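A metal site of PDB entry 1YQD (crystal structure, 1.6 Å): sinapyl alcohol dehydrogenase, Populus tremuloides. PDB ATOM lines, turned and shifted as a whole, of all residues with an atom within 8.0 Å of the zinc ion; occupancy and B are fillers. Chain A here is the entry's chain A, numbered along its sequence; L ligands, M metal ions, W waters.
The side-chain sulfur (SG) of Cys 102 lies within hydrogen-bond range of a ring nitrogen (ND1) of His 76. The side-chain sulfur (SG) of Cys 170 sits close to the side-chain sulfur (SG) of Cys 102 (3.3 Å). OG1 of Thr 174 is in hydrogen-bond range of O of Cys 170 (2.7 Å). N of Ser 56 sits close to SG of Cys 54, at 3.4 Å. The side-chain sulfur (SG) of Cys 54 sits close to the guanidinium group (NH2) of Arg 352. N of Cys 54 sits at hydrogen-bond distance from OD1 of Asp 57 (3.1 Å).
Water W1 is bound to the zinc ion (2.1 Å). A ring nitrogen (NE2) of His 76 binds the zinc ion, 2.2 Å away. SG of Cys 170 is bound to the zinc ion (2.3 Å). The zinc ion is bound by SG of Cys 54.
Merely in contact with the zinc ion: Ser 56.
The side-chain hydroxyl of Ser 56 sits at hydrogen-bond distance from an oxygen (O13) of the ligand, 2.8 Å away. NH1 of Arg 352 is in salt-bridge range of O9 of the ligand, 3.0 Å away. N of His 55 sits at hydrogen-bond distance from O9 of the ligand, at 3.0 Å. O1 of the ligand sits at hydrogen-bond distance from ND1 of His 55 (2.7 Å). The backbone NH (N) of Leu 199 sits at hydrogen-bond distance from an oxygen (O8) of the ligand (2.9 Å). OG1 of Thr 174 lies close to O14 of the ligand. N of Ile 307 is in hydrogen-bond range of O14 of the ligand, at 2.7 Å.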
ATOM      1  N   GLY A  52     -12.599  18.041  -3.352  1.00  0.00           N
ATOM      2  CA  GLY A  52     -13.488  17.278  -2.512  1.00  0.00           C
ATOM      3  C   GLY A  52     -14.501  18.197  -1.868  1.00  0.00           C
ATOM      4  O   GLY A  52     -14.249  19.405  -1.741  1.00  0.00           O
ATOM      5  N   VAL A  53     -15.638  17.643  -1.474  1.00  0.00           N
ATOM      6  CA  VAL A  53     -16.691  18.397  -0.824  1.00  0.00           C
ATOM      7  C   VAL A  53     -16.696  18.015   0.656  1.00  0.00           C
ATOM      8  O   VAL A  53     -17.027  16.889   1.016  1.00  0.00           O
ATOM      9  CB  VAL A  53     -18.063  18.086  -1.447  1.00  0.00           C
ATOM     10  CG1 VAL A  53     -19.170  18.818  -0.685  1.00  0.00           C
ATOM     11  CG2 VAL A  53     -18.080  18.502  -2.912  1.00  0.00           C
ATOM     12  N   CYS A  54     -16.315  18.963   1.504  1.00  0.00           N
ATOM     13  CA  CYS A  54     -16.250  18.740   2.950  1.00  0.00           C
ATOM     14  C   CYS A  54     -17.513  19.268   3.618  1.00  0.00           C
ATOM     15  O   CYS A  54     -18.087  20.245   3.162  1.00  0.00           O
ATOM     16  CB  CYS A  54     -15.017  19.454   3.512  1.00  0.00           C
ATOM     17  SG  CYS A  54     -14.769  19.270   5.298  1.00  0.00           S
ATOM     18  N   HIS A  55     -17.940  18.639   4.701  1.00  0.00           N
ATOM     19  CA  HIS A  55     -19.142  19.123   5.366  1.00  0.00           C
ATOM     20  C   HIS A  55     -18.916  20.569   5.804  1.00  0.00           C
ATOM     21  O   HIS A  55     -19.857  21.328   5.978  1.00  0.00           O
ATOM     22  CB  HIS A  55     -19.513  18.248   6.569  1.00  0.00           C
ATOM     23  CG  HIS A  55     -20.931  18.425   7.028  1.00  0.00           C
ATOM     24  ND1 HIS A  55     -21.819  17.372   7.108  1.00  0.00           N
ATOM     25  CD2 HIS A  55     -21.607  19.520   7.451  1.00  0.00           C
ATOM     26  CE1 HIS A  55     -22.976  17.812   7.572  1.00  0.00           C
ATOM     27  NE2 HIS A  55     -22.875  19.110   7.791  1.00  0.00           N
ATOM     28  N   SER A  56     -17.652  20.952   5.987  1.00  0.00           N
ATOM     29  CA  SER A  56     -17.353  22.325   6.363  1.00  0.00           C
ATOM     30  C   SER A  56     -17.871  23.262   5.281  1.00  0.00           C
ATOM     31  O   SER A  56     -18.308  24.377   5.575  1.00  0.00           O
ATOM     32  CB  SER A  56     -15.856  22.528   6.512  1.00  0.00           C
ATOM     33  OG  SER A  56     -15.398  21.921   7.698  1.00  0.00           O
ATOM     34  N   ASP A  57     -17.810  22.808   4.030  1.00  0.00           N
ATOM     35  CA  ASP A  57     -18.289  23.614   2.905  1.00  0.00           C
ATOM     36  C   ASP A  57     -19.781  23.851   3.114  1.00  0.00           C
ATOM     37  O   ASP A  57     -20.285  24.959   2.891  1.00  0.00           O
ATOM     38  CB  ASP A  57     -18.063  22.875   1.579  1.00  0.00           C
ATOM     39  CG  ASP A  57     -16.579  22.750   1.221  1.00  0.00           C
ATOM     40  OD1 ASP A  57     -16.251  21.872   0.396  1.00  0.00           O
ATOM     41  OD2 ASP A  57     -15.753  23.531   1.743  1.00  0.00           O
ATOM     42  N   TRP A  65     -22.028  28.370  11.451  1.00  0.00           N
ATOM     43  CA  TRP A  65     -21.163  28.880  12.510  1.00  0.00           C
ATOM     44  C   TRP A  65     -21.281  30.379  12.714  1.00  0.00           C
ATOM     45  O   TRP A  65     -20.826  30.899  13.729  1.00  0.00           O
ATOM     46  CB  TRP A  65     -19.705  28.517  12.216  1.00  0.00           C
ATOM     47  CG  TRP A  65     -19.458  27.044  11.983  1.00  0.00           C
ATOM     48  CD1 TRP A  65     -19.922  26.005  12.732  1.00  0.00           C
ATOM     49  CD2 TRP A  65     -18.603  26.482  10.985  1.00  0.00           C
ATOM     50  NE1 TRP A  65     -19.416  24.816  12.256  1.00  0.00           N
ATOM     51  CE2 TRP A  65     -18.594  25.082  11.191  1.00  0.00           C
ATOM     52  CE3 TRP A  65     -17.840  27.010   9.936  1.00  0.00           C
ATOM     53  CZ2 TRP A  65     -17.852  24.210  10.383  1.00  0.00           C
ATOM     54  CZ3 TRP A  65     -17.096  26.144   9.135  1.00  0.00           C
ATOM     55  CH2 TRP A  65     -17.116  24.750   9.370  1.00  0.00           C
ATOM     56  N   GLY A  75     -14.646  24.978  -0.798  1.00  0.00           N
ATOM     57  CA  GLY A  75     -13.748  24.003  -1.365  1.00  0.00           C
ATOM     58  C   GLY A  75     -12.324  24.125  -0.859  1.00  0.00           C
ATOM     59  O   GLY A  75     -11.646  25.102  -1.147  1.00  0.00           O
ATOM     60  N   HIS A  76     -11.876  23.148  -0.076  1.00  0.00           N
ATOM     61  CA  HIS A  76     -10.504  23.181   0.426  1.00  0.00           C
ATOM     62  C   HIS A  76      -9.813  21.811   0.455  1.00  0.00           C
ATOM     63  O   HIS A  76      -8.987  21.516   1.320  1.00  0.00           O
ATOM     64  CB  HIS A  76     -10.413  23.905   1.782  1.00  0.00           C
ATOM     65  CG  HIS A  76     -11.314  23.360   2.839  1.00  0.00           C
ATOM     66  ND1 HIS A  76     -11.716  24.119   3.920  1.00  0.00           N
ATOM     67  CD2 HIS A  76     -11.870  22.139   3.013  1.00  0.00           C
ATOM     68  CE1 HIS A  76     -12.466  23.381   4.718  1.00  0.00           C
ATOM     69  NE2 HIS A  76     -12.573  22.173   4.192  1.00  0.00           N
ATOM     70  N   GLU A  77     -10.176  20.989  -0.521  1.00  0.00           N
ATOM     71  CA  GLU A  77      -9.595  19.659  -0.744  1.00  0.00           C
ATOM     72  C   GLU A  77      -9.346  19.740  -2.237  1.00  0.00           C
ATOM     73  O   GLU A  77      -9.912  18.997  -3.043  1.00  0.00           O
ATOM     74  CB  GLU A  77     -10.609  18.565  -0.381  1.00  0.00           C
ATOM     75  CG  GLU A  77     -10.773  18.410   1.128  1.00  0.00           C
ATOM     76  CD  GLU A  77     -11.786  17.357   1.536  1.00  0.00           C
ATOM     77  OE1 GLU A  77     -11.837  17.023   2.744  1.00  0.00           O
ATOM     78  OE2 GLU A  77     -12.536  16.875   0.669  1.00  0.00           O
ATOM     79  N   GLY A 101      -4.938  22.513   0.900  1.00  0.00           N
ATOM     80  CA  GLY A 101      -5.922  22.137   1.897  1.00  0.00           C
ATOM     81  C   GLY A 101      -6.675  23.324   2.461  1.00  0.00           C
ATOM     82  O   GLY A 101      -7.045  24.236   1.716  1.00  0.00           O
ATOM     83  N   CYS A 102      -6.876  23.328   3.774  1.00  0.00           N
ATOM     84  CA  CYS A 102      -7.617  24.382   4.450  1.00  0.00           C
ATOM     85  C   CYS A 102      -6.875  25.688   4.683  1.00  0.00           C
ATOM     86  O   CYS A 102      -7.492  26.700   5.016  1.00  0.00           O
ATOM     87  CB  CYS A 102      -8.131  23.871   5.803  1.00  0.00           C
ATOM     88  SG  CYS A 102      -9.267  22.504   5.677  1.00  0.00           S
ATOM     89  N   TYR A 128     -10.673  29.624   2.228  1.00  0.00           N
ATOM     90  CA  TYR A 128     -11.833  30.395   1.797  1.00  0.00           C
ATOM     91  C   TYR A 128     -12.514  31.058   2.975  1.00  0.00           C
ATOM     92  O   TYR A 128     -12.437  30.586   4.110  1.00  0.00           O
ATOM     93  CB  TYR A 128     -12.819  29.538   0.990  1.00  0.00           C
ATOM     94  CG  TYR A 128     -13.509  28.422   1.751  1.00  0.00           C
ATOM     95  CD1 TYR A 128     -14.511  28.689   2.678  1.00  0.00           C
ATOM     96  CD2 TYR A 128     -13.176  27.090   1.496  1.00  0.00           C
ATOM     97  CE1 TYR A 128     -15.173  27.653   3.337  1.00  0.00           C
ATOM     98  CE2 TYR A 128     -13.829  26.051   2.155  1.00  0.00           C
ATOM     99  CZ  TYR A 128     -14.826  26.339   3.076  1.00  0.00           C
ATOM    100  OH  TYR A 128     -15.475  25.315   3.707  1.00  0.00           O
ATOM    101  N   PRO A 167      -9.662  14.292  -0.919  1.00  0.00           N
ATOM    102  CA  PRO A 167     -10.179  14.474   0.450  1.00  0.00           C
ATOM    103  C   PRO A 167      -9.125  14.373   1.551  1.00  0.00           C
ATOM    104  O   PRO A 167      -9.361  14.796   2.682  1.00  0.00           O
ATOM    105  CB  PRO A 167     -11.223  13.371   0.572  1.00  0.00           C
ATOM    106  CG  PRO A 167     -11.704  13.199  -0.833  1.00  0.00           C
ATOM    107  CD  PRO A 167     -10.400  13.220  -1.599  1.00  0.00           C
ATOM    108  N   LEU A 169      -6.561  16.040   1.809  1.00  0.00           N
ATOM    109  CA  LEU A 169      -6.094  17.390   2.097  1.00  0.00           C
ATOM    110  C   LEU A 169      -6.782  18.069   3.277  1.00  0.00           C
ATOM    111  O   LEU A 169      -6.224  19.010   3.846  1.00  0.00           O
ATOM    112  CB  LEU A 169      -6.178  18.264   0.844  1.00  0.00           C
ATOM    113  CG  LEU A 169      -5.208  17.802  -0.242  1.00  0.00           C
ATOM    114  CD1 LEU A 169      -5.501  18.504  -1.538  1.00  0.00           C
ATOM    115  CD2 LEU A 169      -3.768  18.075   0.222  1.00  0.00           C
ATOM    116  N   CYS A 170      -7.977  17.619   3.621  1.00  0.00           N
ATOM    117  CA  CYS A 170      -8.657  18.158   4.799  1.00  0.00           C
ATOM    118  C   CYS A 170      -9.057  16.993   5.696  1.00  0.00           C
ATOM    119  O   CYS A 170      -8.570  16.886   6.817  1.00  0.00           O
ATOM    120  CB  CYS A 170      -9.910  18.963   4.456  1.00  0.00           C
ATOM    121  SG  CYS A 170     -10.720  19.567   5.972  1.00  0.00           S
ATOM    122  N   ALA A 171      -9.916  16.116   5.198  1.00  0.00           N
ATOM    123  CA  ALA A 171     -10.354  14.974   5.976  1.00  0.00           C
ATOM    124  C   ALA A 171      -9.175  14.150   6.475  1.00  0.00           C
ATOM    125  O   ALA A 171      -9.095  13.806   7.659  1.00  0.00           O
ATOM    126  CB  ALA A 171     -11.278  14.080   5.145  1.00  0.00           C
ATOM    127  N   THR A 174      -6.818  15.981   9.068  1.00  0.00           N
ATOM    128  CA  THR A 174      -7.586  16.248  10.276  1.00  0.00           C
ATOM    129  C   THR A 174      -7.682  15.056  11.217  1.00  0.00           C
ATOM    130  O   THR A 174      -7.711  15.225  12.437  1.00  0.00           O
ATOM    131  CB  THR A 174      -9.016  16.754   9.925  1.00  0.00           C
ATOM    132  OG1 THR A 174      -8.915  18.019   9.257  1.00  0.00           O
ATOM    133  CG2 THR A 174      -9.844  16.939  11.192  1.00  0.00           C
ATOM    134  N   LEU A 199     -14.662  12.319   7.108  1.00  0.00           N
ATOM    135  CA  LEU A 199     -13.494  12.202   7.965  1.00  0.00           C
ATOM    136  C   LEU A 199     -13.458  10.824   8.604  1.00  0.00           C
ATOM    137  O   LEU A 199     -12.407  10.192   8.698  1.00  0.00           O
ATOM    138  CB  LEU A 199     -13.533  13.255   9.079  1.00  0.00           C
ATOM    139  CG  LEU A 199     -12.875  14.607   8.834  1.00  0.00           C
ATOM    140  CD1 LEU A 199     -13.575  15.352   7.694  1.00  0.00           C
ATOM    141  CD2 LEU A 199     -12.929  15.414  10.126  1.00  0.00           C
ATOM    142  N   ILE A 307      -7.398  20.435  11.652  1.00  0.00           N
ATOM    143  CA  ILE A 307      -6.570  20.070  10.502  1.00  0.00           C
ATOM    144  C   ILE A 307      -5.147  19.656  10.922  1.00  0.00           C
ATOM    145  O   ILE A 307      -4.977  18.761  11.742  1.00  0.00           O
ATOM    146  CB  ILE A 307      -6.519  21.221   9.446  1.00  0.00           C
ATOM    147  CG1 ILE A 307      -6.081  22.545  10.088  1.00  0.00           C
ATOM    148  CG2 ILE A 307      -7.894  21.392   8.821  1.00  0.00           C
ATOM    149  CD1 ILE A 307      -5.928  23.683   9.072  1.00  0.00           C
ATOM    150  N   ARG A 352     -17.497  10.330   0.320  1.00  0.00           N
ATOM    151  CA  ARG A 352     -17.044  11.690   0.049  1.00  0.00           C
ATOM    152  C   ARG A 352     -17.326  12.076  -1.392  1.00  0.00           C
ATOM    153  O   ARG A 352     -17.009  11.330  -2.315  1.00  0.00           O
ATOM    154  CB  ARG A 352     -15.527  11.796   0.277  1.00  0.00           C
ATOM    155  CG  ARG A 352     -15.092  12.723   1.413  1.00  0.00           C
ATOM    156  CD  ARG A 352     -15.171  14.193   1.014  1.00  0.00           C
ATOM    157  NE  ARG A 352     -14.435  15.072   1.917  1.00  0.00           N
ATOM    158  CZ  ARG A 352     -14.830  15.383   3.158  1.00  0.00           C
ATOM    159  NH1 ARG A 352     -15.951  14.886   3.633  1.00  0.00           N
ATOM    160  NH2 ARG A 352     -14.102  16.206   3.895  1.00  0.00           N
HETATM  161  P1  LIG L   1     -20.089  14.106   6.906  1.00  0.00           P
HETATM  162  O1  LIG L   1     -21.380  14.675   6.911  1.00  0.00           O
HETATM  163  O2  LIG L   1     -19.447  13.452   5.729  1.00  0.00           O
HETATM  164  O3  LIG L   1     -19.923  12.991   8.040  1.00  0.00           O
HETATM  165  C1  LIG L   1     -20.456  13.283   9.330  1.00  0.00           C
HETATM  166  C2  LIG L   1     -20.700  11.840   9.756  1.00  0.00           C
HETATM  167  O4  LIG L   1     -21.403  11.880  11.240  1.00  0.00           O
HETATM  168  C3  LIG L   1     -22.237  11.346   9.238  1.00  0.00           C
HETATM  169  O5  LIG L   1     -21.771  10.296   8.247  1.00  0.00           O
HETATM  170  C4  LIG L   1     -22.895  10.502  10.227  1.00  0.00           C
HETATM  171  O6  LIG L   1     -22.214   9.311  10.507  1.00  0.00           O
HETATM  172  C5  LIG L   1     -22.525  11.401  11.511  1.00  0.00           C
HETATM  173  N1  LIG L   1     -23.656  12.294  11.830  1.00  0.00           N
HETATM  174  C6  LIG L   1     -24.268  13.310  11.093  1.00  0.00           C
HETATM  175  N2  LIG L   1     -25.270  13.897  11.754  1.00  0.00           N
HETATM  176  C7  LIG L   1     -25.300  13.227  12.992  1.00  0.00           C
HETATM  177  C8  LIG L   1     -26.154  13.401  14.153  1.00  0.00           C
HETATM  178  N3  LIG L   1     -27.167  14.289  14.300  1.00  0.00           N
HETATM  179  N4  LIG L   1     -25.926  12.542  15.278  1.00  0.00           N
HETATM  180  C9  LIG L   1     -24.891  11.562  15.261  1.00  0.00           C
HETATM  181  N5  LIG L   1     -24.039  11.379  14.135  1.00  0.00           N
HETATM  182  C10 LIG L   1     -24.288  12.236  13.031  1.00  0.00           C
HETATM  183  O7  LIG L   1     -19.039  15.213   7.372  1.00  0.00           O
HETATM  184  P2  LIG L   1     -17.483  15.195   7.147  1.00  0.00           P
HETATM  185  O8  LIG L   1     -16.654  14.265   7.864  1.00  0.00           O
HETATM  186  O9  LIG L   1     -17.021  16.168   6.146  1.00  0.00           O
HETATM  187  O10 LIG L   1     -17.308  16.315   8.325  1.00  0.00           O
HETATM  188  C11 LIG L   1     -17.640  16.032   9.744  1.00  0.00           C
HETATM  189  C12 LIG L   1     -17.431  17.239  10.651  1.00  0.00           C
HETATM  190  O11 LIG L   1     -16.038  17.552  10.864  1.00  0.00           O
HETATM  191  C13 LIG L   1     -18.059  18.615  10.211  1.00  0.00           C
HETATM  192  O12 LIG L   1     -18.690  19.276  11.339  1.00  0.00           O
HETATM  193  C14 LIG L   1     -16.880  19.356   9.671  1.00  0.00           C
HETATM  194  O13 LIG L   1     -17.093  20.749   9.587  1.00  0.00           O
HETATM  195  C15 LIG L   1     -15.859  18.964  10.628  1.00  0.00           C
HETATM  196  N6  LIG L   1     -14.431  19.110  10.250  1.00  0.00           N
HETATM  197  C16 LIG L   1     -13.498  19.571  11.213  1.00  0.00           C
HETATM  198  C17 LIG L   1     -12.171  19.726  10.851  1.00  0.00           C
HETATM  199  C18 LIG L   1     -11.207  20.218  11.914  1.00  0.00           C
HETATM  200  O14 LIG L   1     -10.054  20.371  11.582  1.00  0.00           O
HETATM  201  N7  LIG L   1     -11.618  20.470  13.116  1.00  0.00           N
HETATM  202  C19 LIG L   1     -11.715  19.420   9.497  1.00  0.00           C
HETATM  203  C20 LIG L   1     -12.679  18.958   8.555  1.00  0.00           C
HETATM  204  C21 LIG L   1     -14.062  18.789   8.903  1.00  0.00           C
HETATM  205  P3  LIG L   1     -23.089   7.905  10.865  1.00  0.00           P
HETATM  206  O15 LIG L   1     -22.007   6.844  11.069  1.00  0.00           O
HETATM  207  O16 LIG L   1     -23.831   8.273  12.113  1.00  0.00           O
HETATM  208  O17 LIG L   1     -23.946   7.613   9.641  1.00  0.00           O
HETATM  209 ZN    ZN M   1     -12.812  20.560   5.614  1.00  0.00          ZN
HETATM  210  O   HOH W   1     -12.925  21.664   7.376  1.00  0.00           O
